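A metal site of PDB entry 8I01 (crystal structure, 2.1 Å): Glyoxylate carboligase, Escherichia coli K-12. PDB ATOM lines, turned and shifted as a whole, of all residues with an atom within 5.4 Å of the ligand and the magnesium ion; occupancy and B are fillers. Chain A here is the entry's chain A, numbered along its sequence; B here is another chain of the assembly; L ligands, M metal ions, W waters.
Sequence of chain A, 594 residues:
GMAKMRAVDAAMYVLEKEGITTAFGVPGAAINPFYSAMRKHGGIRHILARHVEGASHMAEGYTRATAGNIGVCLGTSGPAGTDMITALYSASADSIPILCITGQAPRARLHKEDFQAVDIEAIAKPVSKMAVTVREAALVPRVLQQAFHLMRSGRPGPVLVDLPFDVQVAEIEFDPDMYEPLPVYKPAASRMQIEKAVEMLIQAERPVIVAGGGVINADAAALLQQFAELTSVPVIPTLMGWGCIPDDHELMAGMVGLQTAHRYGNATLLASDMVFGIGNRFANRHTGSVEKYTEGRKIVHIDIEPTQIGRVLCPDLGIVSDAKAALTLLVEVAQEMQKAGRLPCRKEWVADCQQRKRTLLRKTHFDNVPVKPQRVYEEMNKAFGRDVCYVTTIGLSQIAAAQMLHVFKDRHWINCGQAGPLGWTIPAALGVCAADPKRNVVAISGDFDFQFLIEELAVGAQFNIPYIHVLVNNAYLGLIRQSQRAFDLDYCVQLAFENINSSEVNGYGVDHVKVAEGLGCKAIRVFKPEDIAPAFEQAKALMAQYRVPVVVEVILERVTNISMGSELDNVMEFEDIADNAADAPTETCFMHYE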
ATOM      1  N   ILE A 394      -4.239  -6.577   8.559  1.00  0.00           N
ATOM      2  CA  ILE A 394      -5.263  -7.558   8.227  1.00  0.00           C
ATOM      3  C   ILE A 394      -6.257  -6.917   7.283  1.00  0.00           C
ATOM      4  O   ILE A 394      -6.456  -5.696   7.321  1.00  0.00           O
ATOM      5  CB  ILE A 394      -5.975  -8.079   9.512  1.00  0.00           C
ATOM      6  CG1 ILE A 394      -6.907  -9.262   9.202  1.00  0.00           C
ATOM      7  CG2 ILE A 394      -6.739  -6.948  10.146  1.00  0.00           C
ATOM      8  CD1 ILE A 394      -7.387  -9.966  10.463  1.00  0.00           C
ATOM      9  N   GLY A 395      -6.943  -7.740   6.503  1.00  0.00           N
ATOM     10  CA  GLY A 395      -7.872  -7.303   5.478  1.00  0.00           C
ATOM     11  C   GLY A 395      -7.521  -7.928   4.139  1.00  0.00           C
ATOM     12  O   GLY A 395      -6.480  -8.551   3.970  1.00  0.00           O
ATOM     13  N   LEU A 396      -8.420  -7.713   3.168  1.00  0.00           N
ATOM     14  CA  LEU A 396      -8.059  -8.095   1.804  1.00  0.00           C
ATOM     15  C   LEU A 396      -6.819  -7.326   1.340  1.00  0.00           C
ATOM     16  O   LEU A 396      -5.976  -7.870   0.598  1.00  0.00           O
ATOM     17  CB  LEU A 396      -9.229  -7.835   0.858  1.00  0.00           C
ATOM     18  CG  LEU A 396     -10.447  -8.738   1.123  1.00  0.00           C
ATOM     19  CD1 LEU A 396     -11.522  -8.522   0.046  1.00  0.00           C
ATOM     20  CD2 LEU A 396     -10.027 -10.202   1.193  1.00  0.00           C
ATOM     21  N   SER A 397      -6.659  -6.091   1.798  1.00  0.00           N
ATOM     22  CA  SER A 397      -5.448  -5.342   1.528  1.00  0.00           C
ATOM     23  C   SER A 397      -4.212  -6.146   1.919  1.00  0.00           C
ATOM     24  O   SER A 397      -3.241  -6.252   1.148  1.00  0.00           O
ATOM     25  CB  SER A 397      -5.491  -4.054   2.343  1.00  0.00           C
ATOM     26  OG  SER A 397      -5.692  -4.413   3.719  1.00  0.00           O
ATOM     27  N   ALA A 419      -2.915 -12.089  16.074  1.00  0.00           N
ATOM     28  CA  ALA A 419      -4.000 -11.298  16.653  1.00  0.00           C
ATOM     29  C   ALA A 419      -4.656 -10.327  15.673  1.00  0.00           C
ATOM     30  O   ALA A 419      -5.855 -10.069  15.806  1.00  0.00           O
ATOM     31  CB  ALA A 419      -3.501 -10.504  17.866  1.00  0.00           C
ATOM     32  N   GLY A 420      -3.901  -9.763  14.717  1.00  0.00           N
ATOM     33  CA  GLY A 420      -4.498  -8.934  13.680  1.00  0.00           C
ATOM     34  C   GLY A 420      -5.397  -7.779  14.120  1.00  0.00           C
ATOM     35  O   GLY A 420      -6.483  -7.600  13.576  1.00  0.00           O
ATOM     36  N   PRO A 421      -4.982  -6.965  15.092  1.00  0.00           N
ATOM     37  CA  PRO A 421      -5.842  -5.848  15.532  1.00  0.00           C
ATOM     38  C   PRO A 421      -5.870  -4.699  14.534  1.00  0.00           C
ATOM     39  O   PRO A 421      -4.825  -4.129  14.205  1.00  0.00           O
ATOM     40  CB  PRO A 421      -5.188  -5.399  16.852  1.00  0.00           C
ATOM     41  CG  PRO A 421      -3.784  -5.791  16.737  1.00  0.00           C
ATOM     42  CD  PRO A 421      -3.729  -7.019  15.862  1.00  0.00           C
ATOM     43  N   LEU A 422      -7.075  -4.317  14.112  1.00  0.00           N
ATOM     44  CA  LEU A 422      -7.212  -3.173  13.224  1.00  0.00           C
ATOM     45  C   LEU A 422      -6.667  -1.918  13.895  1.00  0.00           C
ATOM     46  O   LEU A 422      -6.772  -1.757  15.113  1.00  0.00           O
ATOM     47  CB  LEU A 422      -8.673  -2.976  12.822  1.00  0.00           C
ATOM     48  CG  LEU A 422      -9.244  -3.979  11.812  1.00  0.00           C
ATOM     49  CD1 LEU A 422     -10.791  -3.877  11.774  1.00  0.00           C
ATOM     50  CD2 LEU A 422      -8.650  -3.785  10.376  1.00  0.00           C
ATOM     51  N   SER A 445      -2.491  -0.550   4.176  1.00  0.00           N
ATOM     52  CA  SER A 445      -3.756  -0.577   4.910  1.00  0.00           C
ATOM     53  C   SER A 445      -4.927  -0.543   3.944  1.00  0.00           C
ATOM     54  O   SER A 445      -4.887   0.172   2.932  1.00  0.00           O
ATOM     55  CB  SER A 445      -3.985   0.640   5.831  1.00  0.00           C
ATOM     56  OG  SER A 445      -3.181   0.578   6.983  1.00  0.00           O
ATOM     57  N   GLY A 446      -6.005  -1.226   4.320  1.00  0.00           N
ATOM     58  CA  GLY A 446      -7.312  -0.889   3.793  1.00  0.00           C
ATOM     59  C   GLY A 446      -7.859   0.348   4.491  1.00  0.00           C
ATOM     60  O   GLY A 446      -7.285   0.852   5.463  1.00  0.00           O
ATOM     61  N   ASP A 447      -8.987   0.854   3.960  1.00  0.00           N
ATOM     62  CA  ASP A 447      -9.521   2.108   4.512  1.00  0.00           C
ATOM     63  C   ASP A 447      -9.982   1.955   5.967  1.00  0.00           C
ATOM     64  O   ASP A 447      -9.779   2.873   6.767  1.00  0.00           O
ATOM     65  CB  ASP A 447     -10.650   2.681   3.634  1.00  0.00           C
ATOM     66  CG  ASP A 447     -11.642   1.625   3.143  1.00  0.00           C
ATOM     67  OD1 ASP A 447     -11.252   0.523   2.712  1.00  0.00           O
ATOM     68  OD2 ASP A 447     -12.858   1.947   3.147  1.00  0.00           O
ATOM     69  N   PHE A 448     -10.557   0.810   6.337  1.00  0.00           N
ATOM     70  CA  PHE A 448     -11.101   0.669   7.684  1.00  0.00           C
ATOM     71  C   PHE A 448      -9.976   0.580   8.726  1.00  0.00           C
ATOM     72  O   PHE A 448     -10.010   1.266   9.743  1.00  0.00           O
ATOM     73  CB  PHE A 448     -12.014  -0.552   7.731  1.00  0.00           C
ATOM     74  CG  PHE A 448     -12.935  -0.638   8.933  1.00  0.00           C
ATOM     75  CD1 PHE A 448     -13.825   0.385   9.246  1.00  0.00           C
ATOM     76  CD2 PHE A 448     -12.962  -1.790   9.706  1.00  0.00           C
ATOM     77  CE1 PHE A 448     -14.703   0.279  10.345  1.00  0.00           C
ATOM     78  CE2 PHE A 448     -13.814  -1.906  10.794  1.00  0.00           C
ATOM     79  CZ  PHE A 448     -14.694  -0.864  11.116  1.00  0.00           C
ATOM     80  N   ASP A 449      -8.956  -0.235   8.452  1.00  0.00           N
ATOM     81  CA  ASP A 449      -7.756  -0.277   9.306  1.00  0.00           C
ATOM     82  C   ASP A 449      -7.138   1.102   9.432  1.00  0.00           C
ATOM     83  O   ASP A 449      -6.694   1.494  10.526  1.00  0.00           O
ATOM     84  CB  ASP A 449      -6.735  -1.274   8.701  1.00  0.00           C
ATOM     85  CG  ASP A 449      -5.325  -1.176   9.307  1.00  0.00           C
ATOM     86  OD1 ASP A 449      -5.151  -1.142  10.549  1.00  0.00           O
ATOM     87  OD2 ASP A 449      -4.346  -1.200   8.539  1.00  0.00           O
ATOM     88  N   PHE A 450      -7.118   1.858   8.341  1.00  0.00           N
ATOM     89  CA  PHE A 450      -6.477   3.175   8.340  1.00  0.00           C
ATOM     90  C   PHE A 450      -7.214   4.138   9.258  1.00  0.00           C
ATOM     91  O   PHE A 450      -6.586   4.995   9.891  1.00  0.00           O
ATOM     92  CB  PHE A 450      -6.441   3.697   6.894  1.00  0.00           C
ATOM     93  CG  PHE A 450      -5.575   4.909   6.696  1.00  0.00           C
ATOM     94  CD1 PHE A 450      -4.203   4.817   6.761  1.00  0.00           C
ATOM     95  CD2 PHE A 450      -6.132   6.128   6.428  1.00  0.00           C
ATOM     96  CE1 PHE A 450      -3.410   5.923   6.568  1.00  0.00           C
ATOM     97  CE2 PHE A 450      -5.341   7.237   6.218  1.00  0.00           C
ATOM     98  CZ  PHE A 450      -3.975   7.130   6.298  1.00  0.00           C
ATOM     99  N   PHE A 452      -9.043   3.443  12.138  1.00  0.00           N
ATOM    100  CA  PHE A 452      -9.089   3.148  13.576  1.00  0.00           C
ATOM    101  C   PHE A 452      -8.204   4.087  14.387  1.00  0.00           C
ATOM    102  O   PHE A 452      -8.635   4.668  15.389  1.00  0.00           O
ATOM    103  CB  PHE A 452      -8.630   1.702  13.846  1.00  0.00           C
ATOM    104  CG  PHE A 452      -9.760   0.676  14.030  1.00  0.00           C
ATOM    105  CD1 PHE A 452     -10.711   0.464  13.047  1.00  0.00           C
ATOM    106  CD2 PHE A 452      -9.793  -0.147  15.175  1.00  0.00           C
ATOM    107  CE1 PHE A 452     -11.724  -0.487  13.205  1.00  0.00           C
ATOM    108  CE2 PHE A 452     -10.786  -1.122  15.338  1.00  0.00           C
ATOM    109  CZ  PHE A 452     -11.754  -1.285  14.354  1.00  0.00           C
ATOM    110  N   VAL A 472      -5.382   1.440   0.290  1.00  0.00           N
ATOM    111  CA  VAL A 472      -6.207   0.922  -0.800  1.00  0.00           C
ATOM    112  C   VAL A 472      -7.661   0.993  -0.335  1.00  0.00           C
ATOM    113  O   VAL A 472      -8.062   0.311   0.621  1.00  0.00           O
ATOM    114  CB  VAL A 472      -5.765  -0.489  -1.237  1.00  0.00           C
ATOM    115  CG1 VAL A 472      -4.335  -0.442  -1.742  1.00  0.00           C
ATOM    116  CG2 VAL A 472      -5.854  -1.516  -0.108  1.00  0.00           C
ATOM    117  N   ASN A 473      -8.452   1.839  -0.982  1.00  0.00           N
ATOM    118  CA  ASN A 473      -9.747   2.271  -0.463  1.00  0.00           C
ATOM    119  C   ASN A 473     -10.851   1.663  -1.311  1.00  0.00           C
ATOM    120  O   ASN A 473     -11.055   2.072  -2.470  1.00  0.00           O
ATOM    121  CB  ASN A 473      -9.829   3.796  -0.449  1.00  0.00           C
ATOM    122  CG  ASN A 473     -11.164   4.327   0.081  1.00  0.00           C
ATOM    123  OD1 ASN A 473     -11.999   3.576   0.572  1.00  0.00           O
ATOM    124  ND2 ASN A 473     -11.348   5.638  -0.001  1.00  0.00           N
ATOM    125  N   ASN A 474     -11.587   0.701  -0.747  1.00  0.00           N
ATOM    126  CA  ASN A 474     -12.769   0.160  -1.392  1.00  0.00           C
ATOM    127  C   ASN A 474     -14.065   0.611  -0.721  1.00  0.00           C
ATOM    128  O   ASN A 474     -15.143   0.148  -1.095  1.00  0.00           O
ATOM    129  CB  ASN A 474     -12.687  -1.374  -1.466  1.00  0.00           C
ATOM    130  CG  ASN A 474     -12.437  -2.034  -0.101  1.00  0.00           C
ATOM    131  OD1 ASN A 474     -12.667  -1.446   0.953  1.00  0.00           O
ATOM    132  ND2 ASN A 474     -11.960  -3.272  -0.135  1.00  0.00           N
ATOM    133  N   ALA A 475     -13.984   1.508   0.265  1.00  0.00           N
ATOM    134  CA  ALA A 475     -15.155   1.933   1.048  1.00  0.00           C
ATOM    135  C   ALA A 475     -15.953   0.722   1.570  1.00  0.00           C
ATOM    136  O   ALA A 475     -17.193   0.745   1.644  1.00  0.00           O
ATOM    137  CB  ALA A 475     -16.049   2.879   0.253  1.00  0.00           C
ATOM    138  N   TYR A 476     -15.236  -0.322   1.974  1.00  0.00           N
ATOM    139  CA  TYR A 476     -15.823  -1.554   2.488  1.00  0.00           C
ATOM    140  C   TYR A 476     -14.937  -2.109   3.595  1.00  0.00           C
ATOM    141  O   TYR A 476     -13.722  -1.871   3.610  1.00  0.00           O
ATOM    142  CB  TYR A 476     -15.897  -2.627   1.390  1.00  0.00           C
ATOM    143  CG  TYR A 476     -17.244  -2.961   0.761  1.00  0.00           C
ATOM    144  CD1 TYR A 476     -18.164  -3.774   1.415  1.00  0.00           C
ATOM    145  CD2 TYR A 476     -17.543  -2.556  -0.530  1.00  0.00           C
ATOM    146  CE1 TYR A 476     -19.360  -4.125   0.814  1.00  0.00           C
ATOM    147  CE2 TYR A 476     -18.740  -2.903  -1.147  1.00  0.00           C
ATOM    148  CZ  TYR A 476     -19.641  -3.690  -0.468  1.00  0.00           C
ATOM    149  OH  TYR A 476     -20.829  -4.036  -1.074  1.00  0.00           O
ATOM    150  N   LEU A 477     -15.530  -2.885   4.512  1.00  0.00           N
ATOM    151  CA  LEU A 477     -14.773  -3.885   5.274  1.00  0.00           C
ATOM    152  C   LEU A 477     -14.650  -5.115   4.374  1.00  0.00           C
ATOM    153  O   LEU A 477     -15.474  -6.032   4.418  1.00  0.00           O
ATOM    154  CB  LEU A 477     -15.435  -4.270   6.586  1.00  0.00           C
ATOM    155  CG  LEU A 477     -16.131  -3.325   7.556  1.00  0.00           C
ATOM    156  CD1 LEU A 477     -16.223  -3.882   8.977  1.00  0.00           C
ATOM    157  CD2 LEU A 477     -15.569  -1.956   7.520  1.00  0.00           C
ATOM    158  N   GLY A 478     -13.646  -5.093   3.500  1.00  0.00           N
ATOM    159  CA  GLY A 478     -13.681  -5.995   2.354  1.00  0.00           C
ATOM    160  C   GLY A 478     -13.574  -7.463   2.745  1.00  0.00           C
ATOM    161  O   GLY A 478     -14.283  -8.305   2.200  1.00  0.00           O
ATOM    162  N   LEU A 479     -12.724  -7.766   3.727  1.00  0.00           N
ATOM    163  CA  LEU A 479     -12.580  -9.158   4.135  1.00  0.00           C
ATOM    164  C   LEU A 479     -13.868  -9.680   4.735  1.00  0.00           C
ATOM    165  O   LEU A 479     -14.238 -10.831   4.491  1.00  0.00           O
ATOM    166  CB  LEU A 479     -11.423  -9.309   5.133  1.00  0.00           C
ATOM    167  CG  LEU A 479     -11.185 -10.712   5.729  1.00  0.00           C
ATOM    168  CD1 LEU A 479     -10.968 -11.771   4.657  1.00  0.00           C
ATOM    169  CD2 LEU A 479      -9.983 -10.687   6.674  1.00  0.00           C
ATOM    170  N   ILE A 480     -14.609  -8.830   5.454  1.00  0.00           N
ATOM    171  CA  ILE A 480     -15.851  -9.284   6.092  1.00  0.00           C
ATOM    172  C   ILE A 480     -16.949  -9.461   5.048  1.00  0.00           C
ATOM    173  O   ILE A 480     -17.749 -10.398   5.121  1.00  0.00           O
ATOM    174  CB  ILE A 480     -16.293  -8.321   7.204  1.00  0.00           C
ATOM    175  CG1 ILE A 480     -15.092  -7.945   8.075  1.00  0.00           C
ATOM    176  CG2 ILE A 480     -17.397  -8.952   8.042  1.00  0.00           C
ATOM    177  CD1 ILE A 480     -14.272  -9.139   8.605  1.00  0.00           C
ATOM    178  N   LEU A 495     -18.776   1.421   4.113  1.00  0.00           N
ATOM    179  CA  LEU A 495     -18.334   2.681   4.701  1.00  0.00           C
ATOM    180  C   LEU A 495     -18.676   3.901   3.837  1.00  0.00           C
ATOM    181  O   LEU A 495     -18.388   5.032   4.245  1.00  0.00           O
ATOM    182  CB  LEU A 495     -16.816   2.620   4.946  1.00  0.00           C
ATOM    183  CG  LEU A 495     -16.381   1.514   5.905  1.00  0.00           C
ATOM    184  CD1 LEU A 495     -14.859   1.377   5.940  1.00  0.00           C
ATOM    185  CD2 LEU A 495     -16.928   1.813   7.331  1.00  0.00           C
ATOM    186  N   VAL B  26     -18.861  -3.754  15.138  1.00  0.00           N
ATOM    187  CA  VAL B  26     -17.931  -3.967  14.043  1.00  0.00           C
ATOM    188  C   VAL B  26     -17.965  -5.463  13.757  1.00  0.00           C
ATOM    189  O   VAL B  26     -17.518  -6.256  14.592  1.00  0.00           O
ATOM    190  CB  VAL B  26     -16.507  -3.507  14.392  1.00  0.00           C
ATOM    191  CG1 VAL B  26     -15.519  -3.907  13.256  1.00  0.00           C
ATOM    192  CG2 VAL B  26     -16.484  -2.009  14.650  1.00  0.00           C
ATOM    193  N   PRO B  27     -18.522  -5.893  12.639  1.00  0.00           N
ATOM    194  CA  PRO B  27     -18.606  -7.326  12.358  1.00  0.00           C
ATOM    195  C   PRO B  27     -17.240  -7.891  11.996  1.00  0.00           C
ATOM    196  O   PRO B  27     -16.262  -7.161  11.764  1.00  0.00           O
ATOM    197  CB  PRO B  27     -19.590  -7.403  11.181  1.00  0.00           C
ATOM    198  CG  PRO B  27     -19.387  -6.123  10.473  1.00  0.00           C
ATOM    199  CD  PRO B  27     -19.030  -5.083  11.518  1.00  0.00           C
ATOM    200  N   GLY B  28     -17.170  -9.220  12.033  1.00  0.00           N
ATOM    201  CA  GLY B  28     -16.004 -10.004  11.643  1.00  0.00           C
ATOM    202  C   GLY B  28     -16.463 -11.432  11.462  1.00  0.00           C
ATOM    203  O   GLY B  28     -17.594 -11.793  11.816  1.00  0.00           O
ATOM    204  N   VAL B  52     -13.508  -0.483  17.397  1.00  0.00           N
ATOM    205  CA  VAL B  52     -14.310  -1.251  18.349  1.00  0.00           C
ATOM    206  C   VAL B  52     -14.453  -0.503  19.666  1.00  0.00           C
ATOM    207  O   VAL B  52     -15.503  -0.560  20.302  1.00  0.00           O
ATOM    208  CB  VAL B  52     -13.712  -2.658  18.553  1.00  0.00           C
ATOM    209  CG1 VAL B  52     -14.307  -3.329  19.791  1.00  0.00           C
ATOM    210  CG2 VAL B  52     -13.962  -3.497  17.305  1.00  0.00           C
ATOM    211  N   THR B  76     -16.085  -9.117  16.900  1.00  0.00           N
ATOM    212  CA  THR B  76     -15.612 -10.447  16.547  1.00  0.00           C
ATOM    213  C   THR B  76     -14.699 -10.971  17.675  1.00  0.00           C
ATOM    214  O   THR B  76     -14.685 -10.427  18.777  1.00  0.00           O
ATOM    215  CB  THR B  76     -14.924 -10.425  15.173  1.00  0.00           C
ATOM    216  OG1 THR B  76     -14.737 -11.771  14.711  1.00  0.00           O
ATOM    217  CG2 THR B  76     -13.528  -9.734  15.233  1.00  0.00           C
ATOM    218  N   PRO B  79      -8.886  -9.490  19.086  1.00  0.00           N
ATOM    219  CA  PRO B  79      -8.635  -8.092  19.466  1.00  0.00           C
ATOM    220  C   PRO B  79      -9.887  -7.245  19.629  1.00  0.00           C
ATOM    221  O   PRO B  79      -9.802  -6.165  20.225  1.00  0.00           O
ATOM    222  CB  PRO B  79      -7.762  -7.565  18.325  1.00  0.00           C
ATOM    223  CG  PRO B  79      -8.266  -8.326  17.166  1.00  0.00           C
ATOM    224  CD  PRO B  79      -8.459  -9.751  17.703  1.00  0.00           C
ATOM    225  N   ALA B  80     -11.025  -7.631  19.051  1.00  0.00           N
ATOM    226  CA  ALA B  80     -12.254  -6.899  19.308  1.00  0.00           C
ATOM    227  C   ALA B  80     -12.626  -6.961  20.783  1.00  0.00           C
ATOM    228  O   ALA B  80     -12.922  -5.930  21.391  1.00  0.00           O
ATOM    229  CB  ALA B  80     -13.398  -7.432  18.437  1.00  0.00           C
ATOM    230  N   ASP B  83     -10.350  -4.842  22.813  1.00  0.00           N
ATOM    231  CA  ASP B  83     -10.670  -3.425  22.600  1.00  0.00           C
ATOM    232  C   ASP B  83     -11.902  -2.962  23.372  1.00  0.00           C
ATOM    233  O   ASP B  83     -12.184  -1.758  23.386  1.00  0.00           O
ATOM    234  CB  ASP B  83     -10.919  -3.155  21.105  1.00  0.00           C
ATOM    235  CG  ASP B  83      -9.615  -2.969  20.279  1.00  0.00           C
ATOM    236  OD1 ASP B  83      -8.493  -2.903  20.832  1.00  0.00           O
ATOM    237  OD2 ASP B  83      -9.755  -2.871  19.042  1.00  0.00           O
ATOM    238  N   GLN B 116      -6.771 -15.618  16.229  1.00  0.00           N
ATOM    239  CA  GLN B 116      -7.555 -14.637  16.984  1.00  0.00           C
ATOM    240  C   GLN B 116      -8.397 -15.270  18.095  1.00  0.00           C
ATOM    241  O   GLN B 116      -9.420 -14.731  18.483  1.00  0.00           O
ATOM    242  CB  GLN B 116      -8.460 -13.816  16.060  1.00  0.00           C
ATOM    243  CG  GLN B 116      -7.682 -12.754  15.292  1.00  0.00           C
ATOM    244  CD  GLN B 116      -8.577 -11.815  14.491  1.00  0.00           C
ATOM    245  OE1 GLN B 116      -9.701 -12.168  14.131  1.00  0.00           O
ATOM    246  NE2 GLN B 116      -8.072 -10.605  14.211  1.00  0.00           N
HETATM  247  N1  LIG L   1     -12.225  -5.644  14.967  1.00  0.00           N
HETATM  248  C1  LIG L   1     -10.907  -5.619  15.267  1.00  0.00           C
HETATM  249  C2  LIG L   1     -10.475  -4.788  16.429  1.00  0.00           C
HETATM  250  N2  LIG L   1      -9.949  -6.301  14.622  1.00  0.00           N
HETATM  251  C3  LIG L   1     -10.318  -7.070  13.584  1.00  0.00           C
HETATM  252  N3  LIG L   1      -9.343  -7.749  12.962  1.00  0.00           N
HETATM  253  C4  LIG L   1     -11.682  -7.135  13.163  1.00  0.00           C
HETATM  254  C5  LIG L   1     -12.573  -6.410  13.921  1.00  0.00           C
HETATM  255  C6  LIG L   1     -12.172  -8.005  12.023  1.00  0.00           C
HETATM  256  N4  LIG L   1     -11.707  -7.553  10.685  1.00  0.00           N
HETATM  257  C7  LIG L   1     -10.680  -8.103  10.053  1.00  0.00           C
HETATM  258  S1  LIG L   1     -10.406  -7.395   8.548  1.00  0.00           S
HETATM  259  C8  LIG L   1     -11.748  -6.329   8.757  1.00  0.00           C
HETATM  260  C9  LIG L   1     -12.343  -6.541   9.971  1.00  0.00           C
HETATM  261  C10 LIG L   1     -13.521  -5.821  10.539  1.00  0.00           C
HETATM  262  C11 LIG L   1     -12.095  -5.303   7.702  1.00  0.00           C
HETATM  263  C12 LIG L   1     -10.876  -4.537   7.245  1.00  0.00           C
HETATM  264  O1  LIG L   1     -11.240  -3.588   6.213  1.00  0.00           O
HETATM  265  P1  LIG L   1     -10.187  -2.676   5.465  1.00  0.00           P
HETATM  266  O2  LIG L   1      -9.067  -2.384   6.434  1.00  0.00           O
HETATM  267  O3  LIG L   1     -10.877  -1.594   4.723  1.00  0.00           O
HETATM  268  O4  LIG L   1      -9.668  -3.728   4.410  1.00  0.00           O
HETATM  269  P2  LIG L   1     -10.242  -4.517   3.165  1.00  0.00           P
HETATM  270  O5  LIG L   1     -11.478  -3.822   2.670  1.00  0.00           O
HETATM  271  O6  LIG L   1      -9.098  -4.488   2.130  1.00  0.00           O
HETATM  272  O7  LIG L   1     -10.528  -5.915   3.680  1.00  0.00           O
HETATM  273 MG    MG M   1     -11.789  -1.598   2.783  1.00  0.00          MG
HETATM  274  O   HOH W   1      -8.679  -4.429  -0.733  1.00  0.00           O
HETATM  275  O   HOH W   2     -15.123  -6.465  15.817  1.00  0.00           O
HETATM  276  O   HOH W   3      -9.663  -1.595   1.559  1.00  0.00           O
HETATM  277  O   HOH W   4      -6.599  -3.240   5.990  1.00  0.00           O
HETATM  278  O   HOH W   5     -10.316 -10.842  12.051  1.00  0.00           O
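CD1 of Ile 394 touches C7 of the ligand, 3.8 Å away.
CA of Gly 395 touches O7 of the ligand, 3.5 Å away.
Leu 422 touches the ligand.
Gly 446 touches the ligand (CA to O2, 3.5 Å).
Phe 452 touches the ligand (CE2 to C2, 3.8 Å).
Leu 477 touches the ligand.
Ile 480 touches the ligand.
Val 26 of chain B touches the ligand.
Pro 27 of chain B touches the ligand.
CG2 of Val 52 of chain B touches N1 of the ligand (3.6 Å).
Thr 76 of chain B touches the ligand.
Pro 79 of chain B touches the ligand (CG to N2, 3.7 Å).
Ala 80 of chain B touches the ligand (N to C2, 3.9 Å).
OD2 of Asp 83 of chain B touches C2 of the ligand, 3.3 Å away.
Hydrophobic or aromatic side chains within 4 Å of the ligand: Ile 394, Leu 396, Leu 422, Phe 448, Phe 452, Leu 477, Leu 479, Ile 480, Val 26 of chain B, Val 52 of chain B and Pro 79 of chain B.
Of the 34 residues printed, 25 come within 4 Å of the ligand.
The nearest printed residue that does not touch the ligand is Pro 421 (4.2 Å).
The backbone NH (N) of Asp 447 sits close to an oxygen (O3) of the ligand, 3.2 Å away.
An oxygen (O7) of the ligand lies within hydrogen-bond range of the backbone NH (N) of Gly 478 (3.2 Å).
The backbone NH (N) of Leu 396 lies within hydrogen-bond range of an oxygen (O7) of the ligand (2.8 Å).
The backbone NH (N) of Leu 479 lies within hydrogen-bond range of an oxygen (O7) of the ligand, 2.9 Å away.
N of Phe 448 sits close to O3 of the ligand.
O of Gly 420 sits at hydrogen-bond distance from N3 of the ligand, 2.9 Å away.
The backbone NH (N) of Ser 397 is in hydrogen-bond range of an oxygen (O6) of the ligand.
An oxygen (O2) of the ligand sits at hydrogen-bond distance from the backbone NH (N) of Asp 449, at 3.0 Å.
The side-chain amide nitrogen of Gln 116 of chain B lies close to a nitrogen (N3) of the ligand.
The magnesium ion is bound by the side-chain amide oxygen of Asn 474 (2.0 Å), the backbone carbonyl oxygen of Tyr 476 (2.1 Å), an oxygen (O3) of the ligand (2.1 Å), the side-chain carboxylate of Asp 447 (2.2 Å), an oxygen (O5) of the ligand (2.2 Å) and water W3 (2.5 Å).
The magnesium ion has six donor atoms within binding distance.
The side-chain carboxylate of Asp 447 lies close to the backbone NH of Ala 475 (3.1 Å).
OD1 of Asn 473 sits close to OD2 of Asp 447 (3.2 Å).
The side-chain amide nitrogen (NE2) of Gln 116 of chain B is in hydrogen-bond range of the backbone carbonyl oxygen (O) of Gly 420, at 3.5 Å.
The side-chain hydroxyl of Ser 397 lies within hydrogen-bond range of the backbone NH of Gly 446 (3.3 Å).
OD2 of Asp 449 sits at hydrogen-bond distance from OG of Ser 445, at 2.6 Å.
The backbone carbonyl oxygen (O) of Ala 419 lies within hydrogen-bond range of the side-chain amide nitrogen (NE2) of Gln 116 of chain B (2.8 Å).
Water W3 lies within hydrogen-bond range of the backbone carbonyl oxygen of Val 472 (2.7 Å), an oxygen (O6) of the ligand (3.0 Å), the side-chain amide nitrogen of Asn 474 (3.3 Å) and the backbone NH of Asp 447 (3.5 Å).
Water W4 lies within hydrogen-bond range of an oxygen (O2) of the ligand (2.6 Å), the backbone NH of Gly 446 (2.7 Å), the side-chain hydroxyl of Ser 397 (2.7 Å) and the backbone carbonyl oxygen of Ile 394 (2.8 Å).
Water W2 lies within hydrogen-bond range of the backbone carbonyl oxygen (O) of Val 26 of chain B, the backbone NH (N) of Thr 76 of chain B and a nitrogen (N1) of the ligand.
Water W5 bridges OE1 of Gln 116 of chain B (2.5 Å) and N3 of the ligand (3.4 Å).
Of the 34 residues printed, 3 come within 4 Å of the magnesium ion.
Along chain A the residues within 4 Å of the magnesium ion span positions 447 to 476.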
